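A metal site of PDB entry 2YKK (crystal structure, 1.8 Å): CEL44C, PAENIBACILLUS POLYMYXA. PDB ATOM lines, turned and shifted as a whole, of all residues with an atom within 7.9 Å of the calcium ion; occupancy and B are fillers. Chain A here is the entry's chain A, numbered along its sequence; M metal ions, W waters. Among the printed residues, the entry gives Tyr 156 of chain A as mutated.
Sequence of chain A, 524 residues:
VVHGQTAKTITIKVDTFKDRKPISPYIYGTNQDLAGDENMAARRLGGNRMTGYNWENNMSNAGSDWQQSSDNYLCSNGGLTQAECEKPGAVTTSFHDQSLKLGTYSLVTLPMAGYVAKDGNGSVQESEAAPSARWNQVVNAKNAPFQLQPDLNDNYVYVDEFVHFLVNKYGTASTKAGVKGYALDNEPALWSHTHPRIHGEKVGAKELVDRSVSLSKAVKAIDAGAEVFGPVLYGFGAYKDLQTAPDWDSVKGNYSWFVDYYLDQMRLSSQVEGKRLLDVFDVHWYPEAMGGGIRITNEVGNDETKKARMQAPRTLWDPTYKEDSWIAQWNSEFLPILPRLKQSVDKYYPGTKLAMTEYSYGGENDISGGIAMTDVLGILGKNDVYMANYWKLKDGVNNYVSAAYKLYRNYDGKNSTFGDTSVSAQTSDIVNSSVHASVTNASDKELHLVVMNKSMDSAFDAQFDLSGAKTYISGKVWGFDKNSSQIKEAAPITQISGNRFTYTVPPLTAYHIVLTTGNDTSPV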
ATOM      1  N   ASN A  54     -17.490   5.454 -25.038  1.00  0.00           N
ATOM      2  CA  ASN A  54     -17.916   4.204 -25.651  1.00  0.00           C
ATOM      3  C   ASN A  54     -19.344   4.019 -25.157  1.00  0.00           C
ATOM      4  O   ASN A  54     -19.559   3.783 -23.999  1.00  0.00           O
ATOM      5  CB  ASN A  54     -16.989   3.069 -25.120  1.00  0.00           C
ATOM      6  CG  ASN A  54     -17.467   1.686 -25.495  1.00  0.00           C
ATOM      7  OD1 ASN A  54     -18.604   1.501 -25.944  1.00  0.00           O
ATOM      8  ND2 ASN A  54     -16.551   0.677 -25.413  1.00  0.00           N
ATOM      9  N   TRP A  55     -20.332   4.138 -26.039  1.00  0.00           N
ATOM     10  CA  TRP A  55     -21.722   4.085 -25.613  1.00  0.00           C
ATOM     11  C   TRP A  55     -22.119   2.736 -25.037  1.00  0.00           C
ATOM     12  O   TRP A  55     -23.063   2.652 -24.240  1.00  0.00           O
ATOM     13  CB  TRP A  55     -22.634   4.489 -26.774  1.00  0.00           C
ATOM     14  CG  TRP A  55     -22.885   3.387 -27.782  1.00  0.00           C
ATOM     15  CD1 TRP A  55     -22.115   3.057 -28.859  1.00  0.00           C
ATOM     16  CD2 TRP A  55     -24.041   2.522 -27.815  1.00  0.00           C
ATOM     17  NE1 TRP A  55     -22.713   2.006 -29.556  1.00  0.00           N
ATOM     18  CE2 TRP A  55     -23.880   1.663 -28.930  1.00  0.00           C
ATOM     19  CE3 TRP A  55     -25.163   2.356 -26.975  1.00  0.00           C
ATOM     20  CZ2 TRP A  55     -24.830   0.668 -29.276  1.00  0.00           C
ATOM     21  CZ3 TRP A  55     -26.126   1.379 -27.305  1.00  0.00           C
ATOM     22  CH2 TRP A  55     -25.944   0.549 -28.470  1.00  0.00           C
ATOM     23  N   GLU A  56     -21.429   1.659 -25.457  1.00  0.00           N
ATOM     24  CA  GLU A  56     -21.789   0.322 -25.008  1.00  0.00           C
ATOM     25  C   GLU A  56     -21.520   0.094 -23.529  1.00  0.00           C
ATOM     26  O   GLU A  56     -22.346  -0.591 -22.882  1.00  0.00           O
ATOM     27  CB  GLU A  56     -21.026  -0.744 -25.815  1.00  0.00           C
ATOM     28  CG  GLU A  56     -21.310  -0.652 -27.335  1.00  0.00           C
ATOM     29  CD  GLU A  56     -20.519  -1.750 -28.084  1.00  0.00           C
ATOM     30  OE1 GLU A  56     -19.609  -2.319 -27.486  1.00  0.00           O
ATOM     31  OE2 GLU A  56     -20.806  -2.043 -29.274  1.00  0.00           O
ATOM     32  N   ASN A  57     -20.414   0.624 -22.985  1.00  0.00           N
ATOM     33  CA  ASN A  57     -20.089   0.372 -21.566  1.00  0.00           C
ATOM     34  C   ASN A  57     -19.916   1.654 -20.748  1.00  0.00           C
ATOM     35  O   ASN A  57     -19.572   1.602 -19.548  1.00  0.00           O
ATOM     36  CB  ASN A  57     -18.798  -0.478 -21.466  1.00  0.00           C
ATOM     37  CG  ASN A  57     -17.572   0.262 -22.030  1.00  0.00           C
ATOM     38  OD1 ASN A  57     -17.624   1.432 -22.410  1.00  0.00           O
ATOM     39  ND2 ASN A  57     -16.423  -0.416 -22.007  1.00  0.00           N
ATOM     40  N   LYS A 118     -12.041   0.926 -24.258  1.00  0.00           N
ATOM     41  CA  LYS A 118     -12.514  -0.455 -24.116  1.00  0.00           C
ATOM     42  C   LYS A 118     -12.797  -0.810 -22.642  1.00  0.00           C
ATOM     43  O   LYS A 118     -13.518  -1.773 -22.371  1.00  0.00           O
ATOM     44  CB  LYS A 118     -11.439  -1.402 -24.706  1.00  0.00           C
ATOM     45  CG  LYS A 118     -11.910  -2.897 -24.867  1.00  0.00           C
ATOM     46  CD  LYS A 118     -10.945  -3.648 -25.837  1.00  0.00           C
ATOM     47  CE  LYS A 118     -11.429  -5.083 -26.016  1.00  0.00           C
ATOM     48  NZ  LYS A 118     -12.683  -5.217 -26.891  1.00  0.00           N
ATOM     49  N   ASN A 136     -11.453   0.188 -28.356  1.00  0.00           N
ATOM     50  CA  ASN A 136     -12.299  -0.397 -29.446  1.00  0.00           C
ATOM     51  C   ASN A 136     -12.280   0.547 -30.647  1.00  0.00           C
ATOM     52  O   ASN A 136     -12.156   1.764 -30.469  1.00  0.00           O
ATOM     53  CB  ASN A 136     -13.724  -0.585 -28.972  1.00  0.00           C
ATOM     54  CG  ASN A 136     -13.886  -1.753 -28.034  1.00  0.00           C
ATOM     55  OD1 ASN A 136     -13.182  -2.747 -28.115  1.00  0.00           O
ATOM     56  ND2 ASN A 136     -14.810  -1.629 -27.091  1.00  0.00           N
ATOM     57  N   GLN A 137     -12.401   0.004 -31.871  1.00  0.00           N
ATOM     58  CA  GLN A 137     -12.403   0.836 -33.085  1.00  0.00           C
ATOM     59  C   GLN A 137     -13.810   1.317 -33.350  1.00  0.00           C
ATOM     60  O   GLN A 137     -14.769   0.561 -33.152  1.00  0.00           O
ATOM     61  CB  GLN A 137     -12.012  -0.014 -34.300  1.00  0.00           C
ATOM     62  CG  GLN A 137     -10.652  -0.538 -34.301  1.00  0.00           C
ATOM     63  CD  GLN A 137     -10.564  -1.561 -35.400  1.00  0.00           C
ATOM     64  OE1 GLN A 137     -10.754  -1.235 -36.563  1.00  0.00           O
ATOM     65  NE2 GLN A 137     -10.423  -2.794 -35.022  1.00  0.00           N
ATOM     66  N   LYS A 142     -22.882  -0.045 -39.269  1.00  0.00           N
ATOM     67  CA  LYS A 142     -22.764  -1.457 -38.938  1.00  0.00           C
ATOM     68  C   LYS A 142     -22.941  -2.393 -40.144  1.00  0.00           C
ATOM     69  O   LYS A 142     -22.238  -3.401 -40.234  1.00  0.00           O
ATOM     70  CB  LYS A 142     -23.759  -1.794 -37.831  1.00  0.00           C
ATOM     71  CG  LYS A 142     -23.455  -3.163 -37.194  1.00  0.00           C
ATOM     72  CD  LYS A 142     -24.498  -3.524 -36.182  1.00  0.00           C
ATOM     73  CE  LYS A 142     -24.000  -4.788 -35.385  1.00  0.00           C
ATOM     74  NZ  LYS A 142     -25.117  -5.299 -34.472  1.00  0.00           N
ATOM     75  N   GLN A 147     -28.514  -4.175 -32.818  1.00  0.00           N
ATOM     76  CA  GLN A 147     -28.845  -4.762 -31.532  1.00  0.00           C
ATOM     77  C   GLN A 147     -29.066  -3.651 -30.531  1.00  0.00           C
ATOM     78  O   GLN A 147     -28.215  -2.775 -30.359  1.00  0.00           O
ATOM     79  CB  GLN A 147     -27.709  -5.699 -31.040  1.00  0.00           C
ATOM     80  CG  GLN A 147     -27.259  -6.810 -32.049  1.00  0.00           C
ATOM     81  CD  GLN A 147     -25.867  -7.443 -31.711  1.00  0.00           C
ATOM     82  OE1 GLN A 147     -24.772  -7.036 -32.253  1.00  0.00           O
ATOM     83  NE2 GLN A 147     -25.876  -8.401 -30.812  1.00  0.00           N
ATOM     84  N   PRO A 150     -25.984  -4.208 -27.556  1.00  0.00           N
ATOM     85  CA  PRO A 150     -24.826  -4.366 -28.452  1.00  0.00           C
ATOM     86  C   PRO A 150     -23.850  -5.411 -27.932  1.00  0.00           C
ATOM     87  O   PRO A 150     -23.799  -5.695 -26.712  1.00  0.00           O
ATOM     88  CB  PRO A 150     -24.174  -2.970 -28.418  1.00  0.00           C
ATOM     89  CG  PRO A 150     -24.516  -2.474 -27.012  1.00  0.00           C
ATOM     90  CD  PRO A 150     -25.970  -2.886 -26.876  1.00  0.00           C
ATOM     91  N   ASP A 151     -23.055  -5.983 -28.841  1.00  0.00           N
ATOM     92  CA  ASP A 151     -22.037  -6.961 -28.484  1.00  0.00           C
ATOM     93  C   ASP A 151     -20.927  -6.300 -27.708  1.00  0.00           C
ATOM     94  O   ASP A 151     -20.177  -5.476 -28.246  1.00  0.00           O
ATOM     95  CB  ASP A 151     -21.435  -7.500 -29.788  1.00  0.00           C
ATOM     96  CG  ASP A 151     -20.519  -8.705 -29.597  1.00  0.00           C
ATOM     97  OD1 ASP A 151     -19.876  -8.940 -28.540  1.00  0.00           O
ATOM     98  OD2 ASP A 151     -20.413  -9.436 -30.609  1.00  0.00           O
ATOM     99  N   LEU A 152     -20.787  -6.689 -26.455  1.00  0.00           N
ATOM    100  CA  LEU A 152     -19.826  -6.017 -25.549  1.00  0.00           C
ATOM    101  C   LEU A 152     -18.425  -6.591 -25.642  1.00  0.00           C
ATOM    102  O   LEU A 152     -17.485  -6.035 -25.032  1.00  0.00           O
ATOM    103  CB  LEU A 152     -20.335  -6.171 -24.096  1.00  0.00           C
ATOM    104  CG  LEU A 152     -21.712  -5.572 -23.759  1.00  0.00           C
ATOM    105  CD1 LEU A 152     -22.010  -5.886 -22.281  1.00  0.00           C
ATOM    106  CD2 LEU A 152     -21.769  -4.076 -24.048  1.00  0.00           C
ATOM    107  N   ASN A 153     -18.288  -7.703 -26.350  1.00  0.00           N
ATOM    108  CA  ASN A 153     -17.018  -8.422 -26.316  1.00  0.00           C
ATOM    109  C   ASN A 153     -16.201  -8.360 -27.575  1.00  0.00           C
ATOM    110  O   ASN A 153     -15.098  -8.909 -27.601  1.00  0.00           O
ATOM    111  CB  ASN A 153     -17.227  -9.874 -25.906  1.00  0.00           C
ATOM    112  CG  ASN A 153     -17.883  -9.993 -24.538  1.00  0.00           C
ATOM    113  OD1 ASN A 153     -18.884 -10.678 -24.393  1.00  0.00           O
ATOM    114  ND2 ASN A 153     -17.369  -9.270 -23.568  1.00  0.00           N
ATOM    115  N   ASP A 154     -16.700  -7.706 -28.620  1.00  0.00           N
ATOM    116  CA  ASP A 154     -15.908  -7.556 -29.840  1.00  0.00           C
ATOM    117  C   ASP A 154     -15.077  -6.276 -29.750  1.00  0.00           C
ATOM    118  O   ASP A 154     -15.034  -5.631 -28.678  1.00  0.00           O
ATOM    119  CB  ASP A 154     -16.821  -7.600 -31.081  1.00  0.00           C
ATOM    120  CG  ASP A 154     -17.798  -6.426 -31.167  1.00  0.00           C
ATOM    121  OD1 ASP A 154     -17.693  -5.478 -30.358  1.00  0.00           O
ATOM    122  OD2 ASP A 154     -18.687  -6.434 -32.104  1.00  0.00           O
ATOM    123  N   ASN A 155     -14.406  -5.918 -30.854  1.00  0.00           N
ATOM    124  CA  ASN A 155     -13.498  -4.818 -30.838  1.00  0.00           C
ATOM    125  C   ASN A 155     -14.084  -3.537 -31.436  1.00  0.00           C
ATOM    126  O   ASN A 155     -13.320  -2.642 -31.837  1.00  0.00           O
ATOM    127  CB  ASN A 155     -12.222  -5.211 -31.594  1.00  0.00           C
ATOM    128  CG  ASN A 155     -11.024  -4.470 -31.077  1.00  0.00           C
ATOM    129  OD1 ASN A 155     -10.764  -4.467 -29.874  1.00  0.00           O
ATOM    130  ND2 ASN A 155     -10.322  -3.766 -31.976  1.00  0.00           N
ATOM    131  N   TYR A 156     -15.439  -3.454 -31.494  1.00  0.00           N
ATOM    132  CA  TYR A 156     -16.074  -2.400 -32.311  1.00  0.00           C
ATOM    133  C   TYR A 156     -17.142  -1.705 -31.544  1.00  0.00           C
ATOM    134  O   TYR A 156     -17.756  -2.290 -30.633  1.00  0.00           O
ATOM    135  CB  TYR A 156     -16.794  -3.015 -33.543  1.00  0.00           C
ATOM    136  CG  TYR A 156     -15.816  -3.736 -34.463  1.00  0.00           C
ATOM    137  CD1 TYR A 156     -14.913  -2.973 -35.217  1.00  0.00           C
ATOM    138  CD2 TYR A 156     -15.732  -5.163 -34.480  1.00  0.00           C
ATOM    139  CE1 TYR A 156     -13.949  -3.628 -36.054  1.00  0.00           C
ATOM    140  CE2 TYR A 156     -14.771  -5.800 -35.279  1.00  0.00           C
ATOM    141  CZ  TYR A 156     -13.931  -5.047 -36.061  1.00  0.00           C
ATOM    142  OH  TYR A 156     -12.951  -5.607 -36.833  1.00  0.00           O
ATOM    143  N   VAL A 157     -17.345  -0.440 -31.863  1.00  0.00           N
ATOM    144  CA  VAL A 157     -18.565   0.228 -31.500  1.00  0.00           C
ATOM    145  C   VAL A 157     -19.106   0.800 -32.847  1.00  0.00           C
ATOM    146  O   VAL A 157     -18.325   1.298 -33.635  1.00  0.00           O
ATOM    147  CB  VAL A 157     -18.239   1.281 -30.436  1.00  0.00           C
ATOM    148  CG1 VAL A 157     -19.401   2.183 -30.178  1.00  0.00           C
ATOM    149  CG2 VAL A 157     -17.672   0.599 -29.125  1.00  0.00           C
ATOM    150  N   TYR A 158     -20.409   0.696 -33.063  1.00  0.00           N
ATOM    151  CA  TYR A 158     -20.992   1.138 -34.313  1.00  0.00           C
ATOM    152  C   TYR A 158     -21.845   2.372 -34.042  1.00  0.00           C
ATOM    153  O   TYR A 158     -22.770   2.292 -33.223  1.00  0.00           O
ATOM    154  CB  TYR A 158     -21.934   0.043 -34.842  1.00  0.00           C
ATOM    155  CG  TYR A 158     -21.151  -1.218 -35.212  1.00  0.00           C
ATOM    156  CD1 TYR A 158     -20.359  -1.260 -36.363  1.00  0.00           C
ATOM    157  CD2 TYR A 158     -21.199  -2.346 -34.383  1.00  0.00           C
ATOM    158  CE1 TYR A 158     -19.635  -2.419 -36.690  1.00  0.00           C
ATOM    159  CE2 TYR A 158     -20.483  -3.510 -34.711  1.00  0.00           C
ATOM    160  CZ  TYR A 158     -19.724  -3.522 -35.849  1.00  0.00           C
ATOM    161  OH  TYR A 158     -18.997  -4.687 -36.155  1.00  0.00           O
ATOM    162  N   GLU A 161     -25.625   2.245 -34.851  1.00  0.00           N
ATOM    163  CA  GLU A 161     -26.331   1.357 -33.895  1.00  0.00           C
ATOM    164  C   GLU A 161     -26.695   2.160 -32.642  1.00  0.00           C
ATOM    165  O   GLU A 161     -27.783   2.014 -32.073  1.00  0.00           O
ATOM    166  CB  GLU A 161     -25.437   0.162 -33.515  1.00  0.00           C
ATOM    167  CG  GLU A 161     -26.158  -0.874 -32.658  1.00  0.00           C
ATOM    168  CD  GLU A 161     -25.370  -2.155 -32.630  1.00  0.00           C
ATOM    169  OE1 GLU A 161     -24.210  -2.161 -32.120  1.00  0.00           O
ATOM    170  OE2 GLU A 161     -25.956  -3.180 -33.095  1.00  0.00           O
HETATM  171 CA    CA M   1     -19.055  -3.755 -29.383  1.00  0.00          CA
HETATM  172  O   HOH W   1     -20.346  -4.355 -31.357  1.00  0.00           O
HETATM  173  O   HOH W   2     -17.203  -4.057 -27.925  1.00  0.00           O
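OD1 of Asn 136 sits close to O of Asp 154, at 3.5 Å. The side-chain carboxylate (OD1) of Asp 151 sits at hydrogen-bond distance from the backbone NH (N) of Asn 153 (3.0 Å). The side-chain amino group (NZ) of Lys 118 is in hydrogen-bond range of the backbone carbonyl oxygen (O) of Asp 154 (3.0 Å). The backbone NH (N) of Glu 56 is in hydrogen-bond range of the side-chain amide oxygen (OD1) of Asn 54 (2.9 Å).
The calcium ion is bound by O of Tyr 156 (2.3 Å). O of Asp 151 is bound to the calcium ion, 2.3 Å away. Water W2 is bound to the calcium ion. OD1 of Asp 154 binds the calcium ion (2.4 Å). Water W1 binds the calcium ion. The calcium ion is bound by the side-chain carboxylate (OE1) of Glu 56 (2.4 Å). The calcium ion is bound by OE2 of Glu 56 (2.5 Å). The calcium ion has seven donor atoms within binding distance.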
